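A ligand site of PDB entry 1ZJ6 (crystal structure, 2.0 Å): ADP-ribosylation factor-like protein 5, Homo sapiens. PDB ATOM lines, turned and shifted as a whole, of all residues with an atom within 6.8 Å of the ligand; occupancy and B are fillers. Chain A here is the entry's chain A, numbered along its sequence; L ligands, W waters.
OD1 of Asp 25 lies close to O3 of the ligand (3.1 Å). Leu 24 touches the ligand (O to O1, 3.9 Å). Val 129 touches the ligand (CG2 to N4, 3.5 Å). CD1 of Leu 160 touches C9 of the ligand (3.6 Å).
The backbone carbonyl oxygen (O) of Asn 26 is in hydrogen-bond range of the side-chain amino group (NZ) of Lys 126, 2.9 Å away. OD1 of Asp 66 lies within salt-bridge range of NZ of Lys 29. The side-chain amino group (NZ) of Lys 29 sits at hydrogen-bond distance from the backbone carbonyl oxygen (O) of Gly 23, 3.1 Å away. N of Ala 159 is in hydrogen-bond range of OD1 of Asn 125, 3.0 Å away. ND2 of Asn 125 is in hydrogen-bond range of O of Ala 27 (2.9 Å). The side-chain sulfur (SG) of Cys 157 lies within hydrogen-bond range of the side-chain amide oxygen (OD1) of Asn 125, 3.4 Å away. N of Lys 126 sits at hydrogen-bond distance from O of Cys 157 (3.4 Å). The side-chain hydroxyl (OG1) of Thr 161 is in hydrogen-bond range of the backbone carbonyl oxygen (O) of Cys 158, 3.4 Å away.
The backbone NH (N) of Asn 26 is in hydrogen-bond range of an oxygen (O3) of the ligand, at 2.7 Å. The side-chain carboxylate (OD1) of Asp 128 lies within hydrogen-bond range of a nitrogen (N3) of the ligand, 2.7 Å away. An oxygen (O1) of the ligand is in hydrogen-bond range of the backbone NH of Lys 29 (2.8 Å). An oxygen (O1) of the ligand is in salt-bridge range of the side-chain amino group of Lys 29, 2.7 Å away. The backbone NH of Thr 31 is in hydrogen-bond range of an oxygen (O5) of the ligand (2.8 Å). O5 of the ligand is in hydrogen-bond range of OG1 of Thr 31, at 2.7 Å. An oxygen (O2) of the ligand is in hydrogen-bond range of the backbone NH (N) of Thr 30 (3.0 Å). The side-chain hydroxyl of Thr 30 sits at hydrogen-bond distance from an oxygen (O2) of the ligand (2.8 Å). ND2 of Asn 125 sits at hydrogen-bond distance from N2 of the ligand. The backbone NH of Gly 28 lies within hydrogen-bond range of an oxygen (O1) of the ligand. An oxygen (O11) of the ligand is in hydrogen-bond range of the backbone NH (N) of Ala 159, at 3.0 Å. An oxygen (O11) of the ligand lies within hydrogen-bond range of the backbone NH (N) of Lys 126 (3.2 Å). NZ of Lys 126 is in hydrogen-bond range of O8 of the ligand, 3.1 Å away. An oxygen (O1) of the ligand is in hydrogen-bond range of the backbone NH (N) of Ala 27 (3.3 Å). O11 of the ligand sits close to SG of Cys 158, 3.6 Å away.
Water W2 lies within hydrogen-bond range of the side-chain carboxylate (OD2) of Asp 66, an oxygen (O3) of the ligand and the side-chain carboxylate (OD1) of Asp 25. Water W4 lies within hydrogen-bond range of O2 of the ligand (3.0 Å), OG1 of Thr 30 (3.3 Å) and SD of Met 64 (3.6 Å). Water W1 bridges the side-chain amino group (NZ) of Lys 126 and an oxygen (O8) of the ligand.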
ATOM      1  N   GLY A  23     -12.999  24.709  24.548  1.00  0.00           N
ATOM      2  CA  GLY A  23     -12.238  25.656  25.320  1.00  0.00           C
ATOM      3  C   GLY A  23     -12.860  27.011  25.084  1.00  0.00           C
ATOM      4  O   GLY A  23     -13.683  27.177  24.181  1.00  0.00           O
ATOM      5  N   LEU A  24     -12.491  28.001  25.888  1.00  0.00           N
ATOM      6  CA  LEU A  24     -13.035  29.341  25.718  1.00  0.00           C
ATOM      7  C   LEU A  24     -12.500  29.909  24.416  1.00  0.00           C
ATOM      8  O   LEU A  24     -11.500  29.422  23.867  1.00  0.00           O
ATOM      9  CB  LEU A  24     -12.609  30.244  26.880  1.00  0.00           C
ATOM     10  CG  LEU A  24     -12.922  29.784  28.300  1.00  0.00           C
ATOM     11  CD1 LEU A  24     -12.340  30.791  29.292  1.00  0.00           C
ATOM     12  CD2 LEU A  24     -14.415  29.631  28.494  1.00  0.00           C
ATOM     13  N   ASP A  25     -13.167  30.947  23.935  1.00  0.00           N
ATOM     14  CA  ASP A  25     -12.763  31.622  22.710  1.00  0.00           C
ATOM     15  C   ASP A  25     -11.338  32.129  22.895  1.00  0.00           C
ATOM     16  O   ASP A  25     -10.989  32.644  23.955  1.00  0.00           O
ATOM     17  CB  ASP A  25     -13.744  32.767  22.441  1.00  0.00           C
ATOM     18  CG  ASP A  25     -13.419  33.547  21.179  1.00  0.00           C
ATOM     19  OD1 ASP A  25     -12.775  33.014  20.254  1.00  0.00           O
ATOM     20  OD2 ASP A  25     -13.832  34.735  21.106  1.00  0.00           O
ATOM     21  N   ASN A  26     -10.521  31.949  21.869  1.00  0.00           N
ATOM     22  CA  ASN A  26      -9.128  32.386  21.898  1.00  0.00           C
ATOM     23  C   ASN A  26      -8.180  31.513  22.716  1.00  0.00           C
ATOM     24  O   ASN A  26      -7.035  31.889  22.943  1.00  0.00           O
ATOM     25  CB  ASN A  26      -9.049  33.829  22.367  1.00  0.00           C
ATOM     26  CG  ASN A  26      -9.665  34.799  21.368  1.00  0.00           C
ATOM     27  OD1 ASN A  26     -10.412  35.695  21.729  1.00  0.00           O
ATOM     28  ND2 ASN A  26      -9.339  34.600  20.099  1.00  0.00           N
ATOM     29  N   ALA A  27      -8.655  30.359  23.172  1.00  0.00           N
ATOM     30  CA  ALA A  27      -7.807  29.456  23.948  1.00  0.00           C
ATOM     31  C   ALA A  27      -6.688  28.934  23.033  1.00  0.00           C
ATOM     32  O   ALA A  27      -5.581  28.642  23.504  1.00  0.00           O
ATOM     33  CB  ALA A  27      -8.632  28.301  24.495  1.00  0.00           C
ATOM     34  N   GLY A  28      -6.986  28.818  21.749  1.00  0.00           N
ATOM     35  CA  GLY A  28      -6.014  28.339  20.780  1.00  0.00           C
ATOM     36  C   GLY A  28      -6.416  27.068  20.061  1.00  0.00           C
ATOM     37  O   GLY A  28      -5.577  26.375  19.470  1.00  0.00           O
ATOM     38  N   LYS A  29      -7.705  26.762  20.089  1.00  0.00           N
ATOM     39  CA  LYS A  29      -8.228  25.553  19.456  1.00  0.00           C
ATOM     40  C   LYS A  29      -7.963  25.463  17.963  1.00  0.00           C
ATOM     41  O   LYS A  29      -7.498  24.440  17.463  1.00  0.00           O
ATOM     42  CB  LYS A  29      -9.740  25.425  19.715  1.00  0.00           C
ATOM     43  CG  LYS A  29     -10.114  25.411  21.197  1.00  0.00           C
ATOM     44  CD  LYS A  29     -11.616  25.267  21.395  1.00  0.00           C
ATOM     45  CE  LYS A  29     -12.389  26.464  20.857  1.00  0.00           C
ATOM     46  NZ  LYS A  29     -12.021  27.713  21.573  1.00  0.00           N
ATOM     47  N   THR A  30      -8.255  26.540  17.245  1.00  0.00           N
ATOM     48  CA  THR A  30      -8.034  26.560  15.809  1.00  0.00           C
ATOM     49  C   THR A  30      -6.554  26.393  15.456  1.00  0.00           C
ATOM     50  O   THR A  30      -6.207  25.736  14.468  1.00  0.00           O
ATOM     51  CB  THR A  30      -8.572  27.875  15.179  1.00  0.00           C
ATOM     52  OG1 THR A  30      -9.983  27.982  15.444  1.00  0.00           O
ATOM     53  CG2 THR A  30      -8.349  27.894  13.678  1.00  0.00           C
ATOM     54  N   THR A  31      -5.687  26.985  16.277  1.00  0.00           N
ATOM     55  CA  THR A  31      -4.247  26.897  16.037  1.00  0.00           C
ATOM     56  C   THR A  31      -3.768  25.459  16.188  1.00  0.00           C
ATOM     57  O   THR A  31      -2.966  24.975  15.392  1.00  0.00           O
ATOM     58  CB  THR A  31      -3.473  27.815  17.025  1.00  0.00           C
ATOM     59  OG1 THR A  31      -3.976  29.153  16.907  1.00  0.00           O
ATOM     60  CG2 THR A  31      -1.978  27.830  16.700  1.00  0.00           C
ATOM     61  N   ILE A  32      -4.288  24.753  17.194  1.00  0.00           N
ATOM     62  CA  ILE A  32      -3.920  23.359  17.420  1.00  0.00           C
ATOM     63  C   ILE A  32      -4.416  22.485  16.271  1.00  0.00           C
ATOM     64  O   ILE A  32      -3.660  21.644  15.759  1.00  0.00           O
ATOM     65  CB  ILE A  32      -4.505  22.841  18.757  1.00  0.00           C
ATOM     66  CG1 ILE A  32      -3.718  23.452  19.931  1.00  0.00           C
ATOM     67  CG2 ILE A  32      -4.425  21.317  18.814  1.00  0.00           C
ATOM     68  CD1 ILE A  32      -4.439  23.351  21.269  1.00  0.00           C
ATOM     69  N   MET A  64     -15.486  20.708  17.195  1.00  0.00           N
ATOM     70  CA  MET A  64     -14.962  21.855  17.924  1.00  0.00           C
ATOM     71  C   MET A  64     -15.939  22.959  18.264  1.00  0.00           C
ATOM     72  O   MET A  64     -16.813  23.313  17.462  1.00  0.00           O
ATOM     73  CB  MET A  64     -13.809  22.463  17.132  1.00  0.00           C
ATOM     74  CG  MET A  64     -13.270  23.765  17.710  1.00  0.00           C
ATOM     75  SD  MET A  64     -11.806  24.340  16.840  1.00  0.00           S
ATOM     76  CE  MET A  64     -12.535  25.126  15.427  1.00  0.00           C
ATOM     77  N   ASP A  66     -16.602  26.591  21.183  1.00  0.00           N
ATOM     78  CA  ASP A  66     -16.287  27.486  22.275  1.00  0.00           C
ATOM     79  C   ASP A  66     -17.241  27.241  23.412  1.00  0.00           C
ATOM     80  O   ASP A  66     -18.434  27.101  23.207  1.00  0.00           O
ATOM     81  CB  ASP A  66     -16.464  28.939  21.870  1.00  0.00           C
ATOM     82  CG  ASP A  66     -15.395  29.423  20.929  1.00  0.00           C
ATOM     83  OD1 ASP A  66     -14.403  28.694  20.725  1.00  0.00           O
ATOM     84  OD2 ASP A  66     -15.544  30.553  20.417  1.00  0.00           O
ATOM     85  N   VAL A  90      -8.878  22.933  25.690  1.00  0.00           N
ATOM     86  CA  VAL A  90      -7.780  23.849  25.481  1.00  0.00           C
ATOM     87  C   VAL A  90      -7.938  24.998  26.467  1.00  0.00           C
ATOM     88  O   VAL A  90      -9.002  25.632  26.534  1.00  0.00           O
ATOM     89  CB  VAL A  90      -7.749  24.375  24.031  1.00  0.00           C
ATOM     90  CG1 VAL A  90      -6.523  25.244  23.815  1.00  0.00           C
ATOM     91  CG2 VAL A  90      -7.757  23.180  23.059  1.00  0.00           C
ATOM     92  N   ASP A  92      -6.301  28.652  28.004  1.00  0.00           N
ATOM     93  CA  ASP A  92      -5.394  29.770  27.782  1.00  0.00           C
ATOM     94  C   ASP A  92      -4.672  29.949  29.124  1.00  0.00           C
ATOM     95  O   ASP A  92      -5.261  30.433  30.095  1.00  0.00           O
ATOM     96  CB  ASP A  92      -6.183  31.052  27.447  1.00  0.00           C
ATOM     97  CG  ASP A  92      -5.276  32.261  27.255  1.00  0.00           C
ATOM     98  OD1 ASP A  92      -4.069  32.153  27.535  1.00  0.00           O
ATOM     99  OD2 ASP A  92      -5.795  33.320  26.827  1.00  0.00           O
ATOM    100  N   THR A  94      -2.664  32.083  30.152  1.00  0.00           N
ATOM    101  CA  THR A  94      -2.484  33.466  30.583  1.00  0.00           C
ATOM    102  C   THR A  94      -3.771  34.096  31.133  1.00  0.00           C
ATOM    103  O   THR A  94      -3.760  35.239  31.584  1.00  0.00           O
ATOM    104  CB  THR A  94      -2.024  34.369  29.421  1.00  0.00           C
ATOM    105  OG1 THR A  94      -3.102  34.539  28.502  1.00  0.00           O
ATOM    106  CG2 THR A  94      -0.858  33.720  28.685  1.00  0.00           C
ATOM    107  N   ALA A 124      -2.645  22.809  28.269  1.00  0.00           N
ATOM    108  CA  ALA A 124      -2.378  24.087  28.948  1.00  0.00           C
ATOM    109  C   ALA A 124      -1.607  24.861  27.882  1.00  0.00           C
ATOM    110  O   ALA A 124      -0.373  24.796  27.812  1.00  0.00           O
ATOM    111  CB  ALA A 124      -1.496  23.860  30.175  1.00  0.00           C
ATOM    112  N   ASN A 125      -2.339  25.582  27.044  1.00  0.00           N
ATOM    113  CA  ASN A 125      -1.760  26.323  25.928  1.00  0.00           C
ATOM    114  C   ASN A 125      -1.175  27.684  26.281  1.00  0.00           C
ATOM    115  O   ASN A 125      -1.433  28.225  27.353  1.00  0.00           O
ATOM    116  CB  ASN A 125      -2.819  26.446  24.823  1.00  0.00           C
ATOM    117  CG  ASN A 125      -2.223  26.823  23.472  1.00  0.00           C
ATOM    118  OD1 ASN A 125      -1.146  26.350  23.115  1.00  0.00           O
ATOM    119  ND2 ASN A 125      -2.934  27.652  22.724  1.00  0.00           N
ATOM    120  N   LYS A 126      -0.372  28.223  25.371  1.00  0.00           N
ATOM    121  CA  LYS A 126       0.285  29.509  25.560  1.00  0.00           C
ATOM    122  C   LYS A 126       1.251  29.477  26.743  1.00  0.00           C
ATOM    123  O   LYS A 126       1.412  30.468  27.453  1.00  0.00           O
ATOM    124  CB  LYS A 126      -0.778  30.615  25.768  1.00  0.00           C
ATOM    125  CG  LYS A 126      -1.893  30.596  24.717  1.00  0.00           C
ATOM    126  CD  LYS A 126      -2.666  31.909  24.634  1.00  0.00           C
ATOM    127  CE  LYS A 126      -3.773  31.824  23.588  1.00  0.00           C
ATOM    128  NZ  LYS A 126      -4.456  33.117  23.349  1.00  0.00           N
ATOM    129  N   GLN A 127       1.896  28.324  26.933  1.00  0.00           N
ATOM    130  CA  GLN A 127       2.860  28.166  28.019  1.00  0.00           C
ATOM    131  C   GLN A 127       4.163  28.877  27.695  1.00  0.00           C
ATOM    132  O   GLN A 127       5.083  28.929  28.510  1.00  0.00           O
ATOM    133  CB  GLN A 127       3.117  26.677  28.305  1.00  0.00           C
ATOM    134  CG  GLN A 127       2.067  26.019  29.210  1.00  0.00           C
ATOM    135  CD  GLN A 127       2.167  26.487  30.646  1.00  0.00           C
ATOM    136  OE1 GLN A 127       3.242  26.463  31.246  1.00  0.00           O
ATOM    137  NE2 GLN A 127       1.042  26.928  31.210  1.00  0.00           N
ATOM    138  N   ASP A 128       4.233  29.430  26.486  1.00  0.00           N
ATOM    139  CA  ASP A 128       5.404  30.189  26.038  1.00  0.00           C
ATOM    140  C   ASP A 128       5.361  31.614  26.583  1.00  0.00           C
ATOM    141  O   ASP A 128       6.368  32.320  26.599  1.00  0.00           O
ATOM    142  CB  ASP A 128       5.422  30.261  24.521  1.00  0.00           C
ATOM    143  CG  ASP A 128       4.167  30.912  23.964  1.00  0.00           C
ATOM    144  OD1 ASP A 128       3.067  30.335  24.159  1.00  0.00           O
ATOM    145  OD2 ASP A 128       4.260  31.989  23.336  1.00  0.00           O
ATOM    146  N   VAL A 129       4.179  32.051  27.020  1.00  0.00           N
ATOM    147  CA  VAL A 129       3.987  33.406  27.527  1.00  0.00           C
ATOM    148  C   VAL A 129       4.454  33.594  28.961  1.00  0.00           C
ATOM    149  O   VAL A 129       4.062  32.851  29.864  1.00  0.00           O
ATOM    150  CB  VAL A 129       2.507  33.825  27.422  1.00  0.00           C
ATOM    151  CG1 VAL A 129       2.317  35.253  27.933  1.00  0.00           C
ATOM    152  CG2 VAL A 129       2.044  33.709  25.978  1.00  0.00           C
ATOM    153  N   CYS A 157       1.739  23.083  26.457  1.00  0.00           N
ATOM    154  CA  CYS A 157       1.949  23.163  25.024  1.00  0.00           C
ATOM    155  C   CYS A 157       1.990  24.603  24.500  1.00  0.00           C
ATOM    156  O   CYS A 157       1.635  25.541  25.206  1.00  0.00           O
ATOM    157  CB  CYS A 157       0.866  22.387  24.250  1.00  0.00           C
ATOM    158  SG  CYS A 157      -0.817  23.108  24.231  1.00  0.00           S
ATOM    159  N   CYS A 158       2.479  24.747  23.274  1.00  0.00           N
ATOM    160  CA  CYS A 158       2.547  26.033  22.589  1.00  0.00           C
ATOM    161  C   CYS A 158       2.042  25.711  21.183  1.00  0.00           C
ATOM    162  O   CYS A 158       2.767  25.125  20.374  1.00  0.00           O
ATOM    163  CB  CYS A 158       3.975  26.545  22.505  1.00  0.00           C
ATOM    164  SG  CYS A 158       4.109  28.093  21.561  1.00  0.00           S
ATOM    165  N   ALA A 159       0.795  26.073  20.902  1.00  0.00           N
ATOM    166  CA  ALA A 159       0.190  25.782  19.604  1.00  0.00           C
ATOM    167  C   ALA A 159       0.902  26.448  18.435  1.00  0.00           C
ATOM    168  O   ALA A 159       0.815  25.988  17.297  1.00  0.00           O
ATOM    169  CB  ALA A 159      -1.278  26.170  19.621  1.00  0.00           C
ATOM    170  N   LEU A 160       1.623  27.534  18.700  1.00  0.00           N
ATOM    171  CA  LEU A 160       2.339  28.232  17.636  1.00  0.00           C
ATOM    172  C   LEU A 160       3.518  27.422  17.107  1.00  0.00           C
ATOM    173  O   LEU A 160       3.779  27.403  15.901  1.00  0.00           O
ATOM    174  CB  LEU A 160       2.863  29.585  18.132  1.00  0.00           C
ATOM    175  CG  LEU A 160       1.825  30.644  18.482  1.00  0.00           C
ATOM    176  CD1 LEU A 160       2.526  31.899  18.987  1.00  0.00           C
ATOM    177  CD2 LEU A 160       0.978  30.951  17.249  1.00  0.00           C
ATOM    178  N   THR A 161       4.214  26.744  18.005  1.00  0.00           N
ATOM    179  CA  THR A 161       5.373  25.934  17.625  1.00  0.00           C
ATOM    180  C   THR A 161       5.086  24.443  17.532  1.00  0.00           C
ATOM    181  O   THR A 161       5.856  23.697  16.929  1.00  0.00           O
ATOM    182  CB  THR A 161       6.518  26.138  18.632  1.00  0.00           C
ATOM    183  OG1 THR A 161       6.113  25.636  19.911  1.00  0.00           O
ATOM    184  CG2 THR A 161       6.880  27.610  18.748  1.00  0.00           C
HETATM  185  P1  LIG L   1      -9.682  29.559  19.335  1.00  0.00           P
HETATM  186  O1  LIG L   1      -9.699  28.705  20.539  1.00  0.00           O
HETATM  187  O2  LIG L   1      -9.813  28.942  18.075  1.00  0.00           O
HETATM  188  O3  LIG L   1     -10.803  30.716  19.511  1.00  0.00           O
HETATM  189  P2  LIG L   1      -7.176  30.486  18.104  1.00  0.00           P
HETATM  190  O4  LIG L   1      -8.313  30.318  19.292  1.00  0.00           O
HETATM  191  O5  LIG L   1      -6.593  29.175  17.696  1.00  0.00           O
HETATM  192  O6  LIG L   1      -7.889  31.254  17.009  1.00  0.00           O
HETATM  193  O7  LIG L   1      -6.119  31.330  18.856  1.00  0.00           O
HETATM  194  C1  LIG L   1      -6.388  32.666  19.374  1.00  0.00           C
HETATM  195  C2  LIG L   1      -5.214  33.530  19.411  1.00  0.00           C
HETATM  196  O8  LIG L   1      -4.168  32.899  20.305  1.00  0.00           O
HETATM  197  C3  LIG L   1      -4.409  33.694  18.070  1.00  0.00           C
HETATM  198  O9  LIG L   1      -3.898  35.074  18.139  1.00  0.00           O
HETATM  199  C4  LIG L   1      -3.233  32.696  18.113  1.00  0.00           C
HETATM  200  O10 LIG L   1      -2.089  32.879  17.265  1.00  0.00           O
HETATM  201  C5  LIG L   1      -2.861  32.714  19.620  1.00  0.00           C
HETATM  202  N1  LIG L   1      -2.266  31.459  20.171  1.00  0.00           N
HETATM  203  C6  LIG L   1      -2.885  30.113  19.897  1.00  0.00           C
HETATM  204  N2  LIG L   1      -1.912  29.414  20.636  1.00  0.00           N
HETATM  205  C7  LIG L   1      -0.894  30.065  21.213  1.00  0.00           C
HETATM  206  C8  LIG L   1       0.282  29.930  22.036  1.00  0.00           C
HETATM  207  O11 LIG L   1       0.622  28.702  22.393  1.00  0.00           O
HETATM  208  N3  LIG L   1       1.066  30.990  22.432  1.00  0.00           N
HETATM  209  C9  LIG L   1       0.664  32.375  22.005  1.00  0.00           C
HETATM  210  N4  LIG L   1       1.538  33.232  22.498  1.00  0.00           N
HETATM  211  N5  LIG L   1      -0.396  32.535  21.294  1.00  0.00           N
HETATM  212  C10 LIG L   1      -1.131  31.467  20.907  1.00  0.00           C
HETATM  213  P3  LIG L   1      -4.305  36.188  17.047  1.00  0.00           P
HETATM  214  O12 LIG L   1      -5.763  36.293  17.086  1.00  0.00           O
HETATM  215  O13 LIG L   1      -3.659  35.806  15.730  1.00  0.00           O
HETATM  216  O14 LIG L   1      -3.628  37.533  17.600  1.00  0.00           O
HETATM  217  O   HOH W   1      -2.595  34.796  22.466  1.00  0.00           O
HETATM  218  O   HOH W   2     -13.433  30.693  18.789  1.00  0.00           O
HETATM  219  O   HOH W   3       1.159  35.927  21.324  1.00  0.00           O
HETATM  220  O   HOH W   4     -12.514  27.861  17.481  1.00  0.00           O
